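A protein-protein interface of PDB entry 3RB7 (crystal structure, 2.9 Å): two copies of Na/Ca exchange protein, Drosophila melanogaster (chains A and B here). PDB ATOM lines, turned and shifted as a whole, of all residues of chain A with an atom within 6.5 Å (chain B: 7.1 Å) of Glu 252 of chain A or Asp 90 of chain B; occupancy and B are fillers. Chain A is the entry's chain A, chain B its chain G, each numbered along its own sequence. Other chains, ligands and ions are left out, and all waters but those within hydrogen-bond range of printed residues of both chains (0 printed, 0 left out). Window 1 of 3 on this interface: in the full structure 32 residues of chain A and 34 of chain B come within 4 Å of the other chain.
OE2 of Glu 252 of chain A lies close to SD of Met 115 of chain B, at 3.3 Å.
The backbone carbonyl oxygen (O) of Cys 92 of chain B sits at hydrogen-bond distance from the side-chain hydroxyl (OG1) of Thr 52 of chain B (2.8 Å). The backbone NH (N) of Val 21 of chain B lies within hydrogen-bond range of the backbone carbonyl oxygen (O) of Met 115 of chain B.
Glu 252 of chain A touches Asp 90 of chain B (OE2 to OD2, 3.9 Å). Cys 92 of chain B touches Glu 252 of chain A (SG to O, 3.9 Å). Leu 253 of chain A touches Cys 92 of chain B. OG1 of Thr 254 of chain A touches CG2 of Thr 52 of chain B (3.97 Å). OH of Tyr 94 of chain B touches CB of Thr 255 of chain A (3.8 Å).
Of chain B, only Asp 90, Cys 92 and Met 115 come within 4 Å of Glu 252 of chain A. Printed residues of chain A within 4 Å of Tyr 94 of chain B: Thr 255 (3.8 Å). Printed residues of chain B within 4 Å of Leu 253 of chain A: Cys 92 (3.97 Å). Printed residues of chain B within 4 Å of Thr 255 of chain A: Tyr 94 (3.8 Å). Printed residues of chain B within 4 Å of Thr 254 of chain A: Thr 52. Of the printed residues of chain A, Thr 52 of chain B touches Thr 254. Ala 126 of chain A touches none of the printed residues of chain B. The nearest residue of chain B that does not touch Glu 252 of chain A is Thr 52 of chain B (5.1 Å). The nearest residue of chain A that does not touch Asp 90 of chain B is Gly 251 of chain A (5.7 Å). The nearest printed residue of chain A that does not touch Met 115 of chain B is Leu 253 of chain A (7.2 Å).
Of the 9 printed residues of chain A, 4 touch a printed residue of chain B. Hydrophobic or aromatic side chains of chain A that line the printed part of chain B: Leu 253. Of the 15 printed residues of chain B, 5 touch a printed residue of chain A. Among the printed residues, 6 pairs touch across the chains. Among the printed residues, no Asp or Glu carboxylate lies within 4 Å of a Lys or Arg side-chain nitrogen of the other chain.
No position is printed for both chains. Of the 6 pairs that touch across the chains among the printed residues, none has its exchanged pair printed and touching as well.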
ATOM      1  N   ILE A 124      -7.997 -23.531 -12.030  1.00  0.00           N
ATOM      2  CA  ILE A 124      -7.628 -22.115 -11.913  1.00  0.00           C
ATOM      3  C   ILE A 124      -8.107 -21.265 -13.080  1.00  0.00           C
ATOM      4  O   ILE A 124      -7.886 -21.601 -14.246  1.00  0.00           O
ATOM      5  CB  ILE A 124      -6.099 -21.940 -11.817  1.00  0.00           C
ATOM      6  CG1 ILE A 124      -5.570 -22.495 -10.492  1.00  0.00           C
ATOM      7  CG2 ILE A 124      -5.727 -20.483 -11.990  1.00  0.00           C
ATOM      8  CD1 ILE A 124      -4.286 -23.261 -10.641  1.00  0.00           C
ATOM      9  N   PHE A 125      -8.734 -20.141 -12.751  1.00  0.00           N
ATOM     10  CA  PHE A 125      -9.375 -19.286 -13.746  1.00  0.00           C
ATOM     11  C   PHE A 125      -8.842 -17.862 -13.740  1.00  0.00           C
ATOM     12  O   PHE A 125      -8.648 -17.266 -12.679  1.00  0.00           O
ATOM     13  CB  PHE A 125     -10.891 -19.271 -13.521  1.00  0.00           C
ATOM     14  CG  PHE A 125     -11.541 -20.594 -13.771  1.00  0.00           C
ATOM     15  CD1 PHE A 125     -12.134 -20.866 -14.990  1.00  0.00           C
ATOM     16  CD2 PHE A 125     -11.530 -21.579 -12.796  1.00  0.00           C
ATOM     17  CE1 PHE A 125     -12.725 -22.098 -15.226  1.00  0.00           C
ATOM     18  CE2 PHE A 125     -12.110 -22.814 -13.024  1.00  0.00           C
ATOM     19  CZ  PHE A 125     -12.711 -23.074 -14.241  1.00  0.00           C
ATOM     20  N   ALA A 126      -8.626 -17.309 -14.929  1.00  0.00           N
ATOM     21  CA  ALA A 126      -8.096 -15.961 -15.021  1.00  0.00           C
ATOM     22  C   ALA A 126      -8.187 -15.374 -16.419  1.00  0.00           C
ATOM     23  O   ALA A 126      -8.690 -16.007 -17.348  1.00  0.00           O
ATOM     24  CB  ALA A 126      -6.658 -15.946 -14.544  1.00  0.00           C
ATOM     25  N   ASN A 250      -9.804 -18.693  -8.822  1.00  0.00           N
ATOM     26  CA  ASN A 250      -9.335 -17.673  -9.754  1.00  0.00           C
ATOM     27  C   ASN A 250      -7.861 -17.867 -10.026  1.00  0.00           C
ATOM     28  O   ASN A 250      -7.380 -18.995 -10.115  1.00  0.00           O
ATOM     29  CB  ASN A 250      -9.519 -16.275  -9.156  1.00  0.00           C
ATOM     30  CG  ASN A 250     -10.846 -15.624  -9.540  1.00  0.00           C
ATOM     31  OD1 ASN A 250     -11.511 -15.008  -8.697  1.00  0.00           O
ATOM     32  ND2 ASN A 250     -11.228 -15.739 -10.813  1.00  0.00           N
ATOM     33  N   GLY A 251      -7.142 -16.753 -10.139  1.00  0.00           N
ATOM     34  CA  GLY A 251      -5.695 -16.783 -10.280  1.00  0.00           C
ATOM     35  C   GLY A 251      -5.061 -15.416 -10.090  1.00  0.00           C
ATOM     36  O   GLY A 251      -5.609 -14.544  -9.404  1.00  0.00           O
ATOM     37  N   GLU A 252      -3.901 -15.222 -10.711  1.00  0.00           N
ATOM     38  CA  GLU A 252      -3.203 -13.947 -10.620  1.00  0.00           C
ATOM     39  C   GLU A 252      -3.936 -12.814 -11.342  1.00  0.00           C
ATOM     40  O   GLU A 252      -3.771 -11.648 -10.992  1.00  0.00           O
ATOM     41  CB  GLU A 252      -1.752 -14.075 -11.103  1.00  0.00           C
ATOM     42  CG  GLU A 252      -0.810 -14.645 -10.036  1.00  0.00           C
ATOM     43  CD  GLU A 252       0.669 -14.543 -10.404  1.00  0.00           C
ATOM     44  OE1 GLU A 252       1.008 -13.984 -11.475  1.00  0.00           O
ATOM     45  OE2 GLU A 252       1.495 -15.029  -9.606  1.00  0.00           O
ATOM     46  N   LEU A 253      -4.760 -13.155 -12.324  1.00  0.00           N
ATOM     47  CA  LEU A 253      -5.496 -12.144 -13.068  1.00  0.00           C
ATOM     48  C   LEU A 253      -7.017 -12.312 -12.993  1.00  0.00           C
ATOM     49  O   LEU A 253      -7.641 -12.916 -13.875  1.00  0.00           O
ATOM     50  CB  LEU A 253      -5.042 -12.124 -14.520  1.00  0.00           C
ATOM     51  CG  LEU A 253      -3.594 -11.722 -14.750  1.00  0.00           C
ATOM     52  CD1 LEU A 253      -3.474 -11.106 -16.126  1.00  0.00           C
ATOM     53  CD2 LEU A 253      -3.135 -10.735 -13.700  1.00  0.00           C
ATOM     54  N   THR A 254      -7.613 -11.751 -11.947  1.00  0.00           N
ATOM     55  CA  THR A 254      -9.054 -11.829 -11.751  1.00  0.00           C
ATOM     56  C   THR A 254      -9.705 -10.518 -12.176  1.00  0.00           C
ATOM     57  O   THR A 254     -10.930 -10.421 -12.329  1.00  0.00           O
ATOM     58  CB  THR A 254      -9.367 -12.120 -10.294  1.00  0.00           C
ATOM     59  OG1 THR A 254      -8.988 -10.994  -9.488  1.00  0.00           O
ATOM     60  CG2 THR A 254      -8.574 -13.330  -9.853  1.00  0.00           C
ATOM     61  N   THR A 255      -8.860  -9.512 -12.374  1.00  0.00           N
ATOM     62  CA  THR A 255      -9.290  -8.228 -12.903  1.00  0.00           C
ATOM     63  C   THR A 255      -8.520  -7.940 -14.181  1.00  0.00           C
ATOM     64  O   THR A 255      -7.327  -8.253 -14.282  1.00  0.00           O
ATOM     65  CB  THR A 255      -9.036  -7.077 -11.886  1.00  0.00           C
ATOM     66  OG1 THR A 255      -9.947  -7.195 -10.786  1.00  0.00           O
ATOM     67  CG2 THR A 255      -9.206  -5.701 -12.546  1.00  0.00           C
ATOM     68  N   VAL B  21       7.677  -8.051  -6.813  1.00  0.00           N
ATOM     69  CA  VAL B  21       8.227  -7.601  -5.552  1.00  0.00           C
ATOM     70  C   VAL B  21       8.051  -8.613  -4.410  1.00  0.00           C
ATOM     71  O   VAL B  21       7.045  -9.313  -4.333  1.00  0.00           O
ATOM     72  CB  VAL B  21       7.585  -6.269  -5.180  1.00  0.00           C
ATOM     73  CG1 VAL B  21       7.768  -5.979  -3.709  1.00  0.00           C
ATOM     74  CG2 VAL B  21       8.168  -5.163  -6.040  1.00  0.00           C
ATOM     75  N   THR B  52      -5.865  -6.772  -6.461  1.00  0.00           N
ATOM     76  CA  THR B  52      -5.985  -7.838  -5.480  1.00  0.00           C
ATOM     77  C   THR B  52      -5.426  -7.376  -4.122  1.00  0.00           C
ATOM     78  O   THR B  52      -5.772  -7.938  -3.085  1.00  0.00           O
ATOM     79  CB  THR B  52      -5.291  -9.139  -5.969  1.00  0.00           C
ATOM     80  OG1 THR B  52      -4.152  -8.805  -6.771  1.00  0.00           O
ATOM     81  CG2 THR B  52      -6.228  -9.963  -6.824  1.00  0.00           C
ATOM     82  N   PHE B  87       0.492 -14.820   6.194  1.00  0.00           N
ATOM     83  CA  PHE B  87       0.627 -15.402   4.871  1.00  0.00           C
ATOM     84  C   PHE B  87      -0.563 -15.016   4.010  1.00  0.00           C
ATOM     85  O   PHE B  87      -1.711 -15.201   4.418  1.00  0.00           O
ATOM     86  CB  PHE B  87       0.724 -16.918   4.994  1.00  0.00           C
ATOM     87  CG  PHE B  87       0.370 -17.661   3.741  1.00  0.00           C
ATOM     88  CD1 PHE B  87      -0.936 -18.070   3.508  1.00  0.00           C
ATOM     89  CD2 PHE B  87       1.342 -17.980   2.810  1.00  0.00           C
ATOM     90  CE1 PHE B  87      -1.270 -18.772   2.361  1.00  0.00           C
ATOM     91  CE2 PHE B  87       1.014 -18.674   1.665  1.00  0.00           C
ATOM     92  CZ  PHE B  87      -0.296 -19.073   1.441  1.00  0.00           C
ATOM     93  N   GLU B  88      -0.274 -14.461   2.833  1.00  0.00           N
ATOM     94  CA  GLU B  88      -1.283 -14.136   1.827  1.00  0.00           C
ATOM     95  C   GLU B  88      -0.881 -14.811   0.509  1.00  0.00           C
ATOM     96  O   GLU B  88       0.232 -15.343   0.395  1.00  0.00           O
ATOM     97  CB  GLU B  88      -1.388 -12.617   1.644  1.00  0.00           C
ATOM     98  CG  GLU B  88      -1.195 -11.820   2.935  1.00  0.00           C
ATOM     99  CD  GLU B  88      -1.445 -10.319   2.779  1.00  0.00           C
ATOM    100  OE1 GLU B  88      -0.769  -9.515   3.463  1.00  0.00           O
ATOM    101  OE2 GLU B  88      -2.326  -9.946   1.979  1.00  0.00           O
ATOM    102  N   GLU B  89      -1.783 -14.818  -0.473  1.00  0.00           N
ATOM    103  CA  GLU B  89      -1.423 -15.244  -1.832  1.00  0.00           C
ATOM    104  C   GLU B  89      -0.813 -14.063  -2.603  1.00  0.00           C
ATOM    105  O   GLU B  89      -0.878 -12.915  -2.151  1.00  0.00           O
ATOM    106  CB  GLU B  89      -2.634 -15.817  -2.586  1.00  0.00           C
ATOM    107  CG  GLU B  89      -2.889 -17.319  -2.375  1.00  0.00           C
ATOM    108  CD  GLU B  89      -3.834 -17.934  -3.420  1.00  0.00           C
ATOM    109  OE1 GLU B  89      -4.725 -17.216  -3.932  1.00  0.00           O
ATOM    110  OE2 GLU B  89      -3.688 -19.146  -3.720  1.00  0.00           O
ATOM    111  N   ASP B  90      -0.213 -14.333  -3.759  1.00  0.00           N
ATOM    112  CA  ASP B  90       0.393 -13.255  -4.540  1.00  0.00           C
ATOM    113  C   ASP B  90      -0.690 -12.323  -5.093  1.00  0.00           C
ATOM    114  O   ASP B  90      -1.738 -12.791  -5.546  1.00  0.00           O
ATOM    115  CB  ASP B  90       1.262 -13.829  -5.657  1.00  0.00           C
ATOM    116  CG  ASP B  90       2.173 -14.953  -5.169  1.00  0.00           C
ATOM    117  OD1 ASP B  90       2.725 -14.853  -4.038  1.00  0.00           O
ATOM    118  OD2 ASP B  90       2.327 -15.941  -5.926  1.00  0.00           O
ATOM    119  N   GLU B  91      -0.448 -11.010  -5.054  1.00  0.00           N
ATOM    120  CA  GLU B  91      -1.496 -10.043  -5.402  1.00  0.00           C
ATOM    121  C   GLU B  91      -1.089  -8.866  -6.317  1.00  0.00           C
ATOM    122  O   GLU B  91      -0.487  -7.901  -5.856  1.00  0.00           O
ATOM    123  CB  GLU B  91      -2.120  -9.496  -4.120  1.00  0.00           C
ATOM    124  CG  GLU B  91      -2.497 -10.562  -3.124  1.00  0.00           C
ATOM    125  CD  GLU B  91      -3.095  -9.977  -1.869  1.00  0.00           C
ATOM    126  OE1 GLU B  91      -2.932  -8.760  -1.650  1.00  0.00           O
ATOM    127  OE2 GLU B  91      -3.727 -10.726  -1.100  1.00  0.00           O
ATOM    128  N   CYS B  92      -1.450  -8.941  -7.600  1.00  0.00           N
ATOM    129  CA  CYS B  92      -1.240  -7.827  -8.526  1.00  0.00           C
ATOM    130  C   CYS B  92      -2.045  -6.587  -8.103  1.00  0.00           C
ATOM    131  O   CYS B  92      -3.276  -6.596  -8.169  1.00  0.00           O
ATOM    132  CB  CYS B  92      -1.653  -8.207  -9.969  1.00  0.00           C
ATOM    133  SG  CYS B  92      -0.630  -9.419 -10.913  1.00  0.00           S
ATOM    134  N   TYR B  94      -2.117  -2.106  -8.817  1.00  0.00           N
ATOM    135  CA  TYR B  94      -2.011  -1.323 -10.049  1.00  0.00           C
ATOM    136  C   TYR B  94      -1.634   0.149  -9.859  1.00  0.00           C
ATOM    137  O   TYR B  94      -2.255   0.847  -9.057  1.00  0.00           O
ATOM    138  CB  TYR B  94      -3.343  -1.401 -10.809  1.00  0.00           C
ATOM    139  CG  TYR B  94      -3.887  -2.809 -10.968  1.00  0.00           C
ATOM    140  CD1 TYR B  94      -5.226  -3.098 -10.721  1.00  0.00           C
ATOM    141  CD2 TYR B  94      -3.056  -3.853 -11.366  1.00  0.00           C
ATOM    142  CE1 TYR B  94      -5.722  -4.391 -10.870  1.00  0.00           C
ATOM    143  CE2 TYR B  94      -3.536  -5.143 -11.514  1.00  0.00           C
ATOM    144  CZ  TYR B  94      -4.868  -5.408 -11.268  1.00  0.00           C
ATOM    145  OH  TYR B  94      -5.326  -6.697 -11.424  1.00  0.00           O
ATOM    146  N   THR B 113       1.271  -2.655 -14.015  1.00  0.00           N
ATOM    147  CA  THR B 113       0.733  -3.660 -13.114  1.00  0.00           C
ATOM    148  C   THR B 113       1.860  -4.057 -12.179  1.00  0.00           C
ATOM    149  O   THR B 113       3.019  -4.082 -12.586  1.00  0.00           O
ATOM    150  CB  THR B 113       0.229  -4.903 -13.867  1.00  0.00           C
ATOM    151  OG1 THR B 113      -0.979  -4.590 -14.584  1.00  0.00           O
ATOM    152  CG2 THR B 113      -0.033  -6.053 -12.877  1.00  0.00           C
ATOM    153  N   MET B 115       2.982  -6.833  -8.855  1.00  0.00           N
ATOM    154  CA  MET B 115       2.632  -7.966  -8.008  1.00  0.00           C
ATOM    155  C   MET B 115       3.376  -7.959  -6.680  1.00  0.00           C
ATOM    156  O   MET B 115       4.527  -7.530  -6.602  1.00  0.00           O
ATOM    157  CB  MET B 115       2.847  -9.300  -8.717  1.00  0.00           C
ATOM    158  CG  MET B 115       1.715 -10.278  -8.462  1.00  0.00           C
ATOM    159  SD  MET B 115       2.221 -11.999  -8.521  1.00  0.00           S
ATOM    160  CE  MET B 115       3.077 -12.062 -10.094  1.00  0.00           C
ATOM    161  N   ILE B 116       2.706  -8.428  -5.634  1.00  0.00           N
ATOM    162  CA  ILE B 116       3.340  -8.570  -4.333  1.00  0.00           C
ATOM    163  C   ILE B 116       3.546 -10.047  -3.994  1.00  0.00           C
ATOM    164  O   ILE B 116       2.600 -10.833  -3.927  1.00  0.00           O
ATOM    165  CB  ILE B 116       2.571  -7.811  -3.228  1.00  0.00           C
ATOM    166  CG1 ILE B 116       3.288  -6.495  -2.918  1.00  0.00           C
ATOM    167  CG2 ILE B 116       2.448  -8.657  -1.960  1.00  0.00           C
ATOM    168  CD1 ILE B 116       2.371  -5.362  -2.471  1.00  0.00           C
ATOM    169  N   LEU B 117       4.806 -10.420  -3.818  1.00  0.00           N
ATOM    170  CA  LEU B 117       5.149 -11.796  -3.541  1.00  0.00           C
ATOM    171  C   LEU B 117       5.257 -12.012  -2.040  1.00  0.00           C
ATOM    172  O   LEU B 117       6.205 -11.562  -1.382  1.00  0.00           O
ATOM    173  CB  LEU B 117       6.429 -12.202  -4.272  1.00  0.00           C
ATOM    174  CG  LEU B 117       6.341 -12.176  -5.800  1.00  0.00           C
ATOM    175  CD1 LEU B 117       7.489 -12.953  -6.384  1.00  0.00           C
ATOM    176  CD2 LEU B 117       5.023 -12.750  -6.301  1.00  0.00           C
ATOM    177  N   ASP B 118       4.242 -12.686  -1.513  1.00  0.00           N
ATOM    178  CA  ASP B 118       4.178 -13.047  -0.115  1.00  0.00           C
ATOM    179  C   ASP B 118       5.408 -13.868   0.247  1.00  0.00           C
ATOM    180  O   ASP B 118       5.775 -14.804  -0.472  1.00  0.00           O
ATOM    181  CB  ASP B 118       2.909 -13.858   0.138  1.00  0.00           C
ATOM    182  CG  ASP B 118       2.807 -14.349   1.561  1.00  0.00           C
ATOM    183  OD1 ASP B 118       2.939 -13.515   2.479  1.00  0.00           O
ATOM    184  OD2 ASP B 118       2.601 -15.568   1.762  1.00  0.00           O
ATOM    185  N   ASP B 119       6.038 -13.510   1.364  1.00  0.00           N
ATOM    186  CA  ASP B 119       7.211 -14.222   1.881  1.00  0.00           C
ATOM    187  C   ASP B 119       6.864 -15.086   3.106  1.00  0.00           C
ATOM    188  O   ASP B 119       7.742 -15.716   3.708  1.00  0.00           O
ATOM    189  CB  ASP B 119       8.287 -13.209   2.264  1.00  0.00           C
ATOM    190  CG  ASP B 119       7.759 -12.142   3.195  1.00  0.00           C
ATOM    191  OD1 ASP B 119       6.736 -11.509   2.840  1.00  0.00           O
ATOM    192  OD2 ASP B 119       8.352 -11.940   4.281  1.00  0.00           O
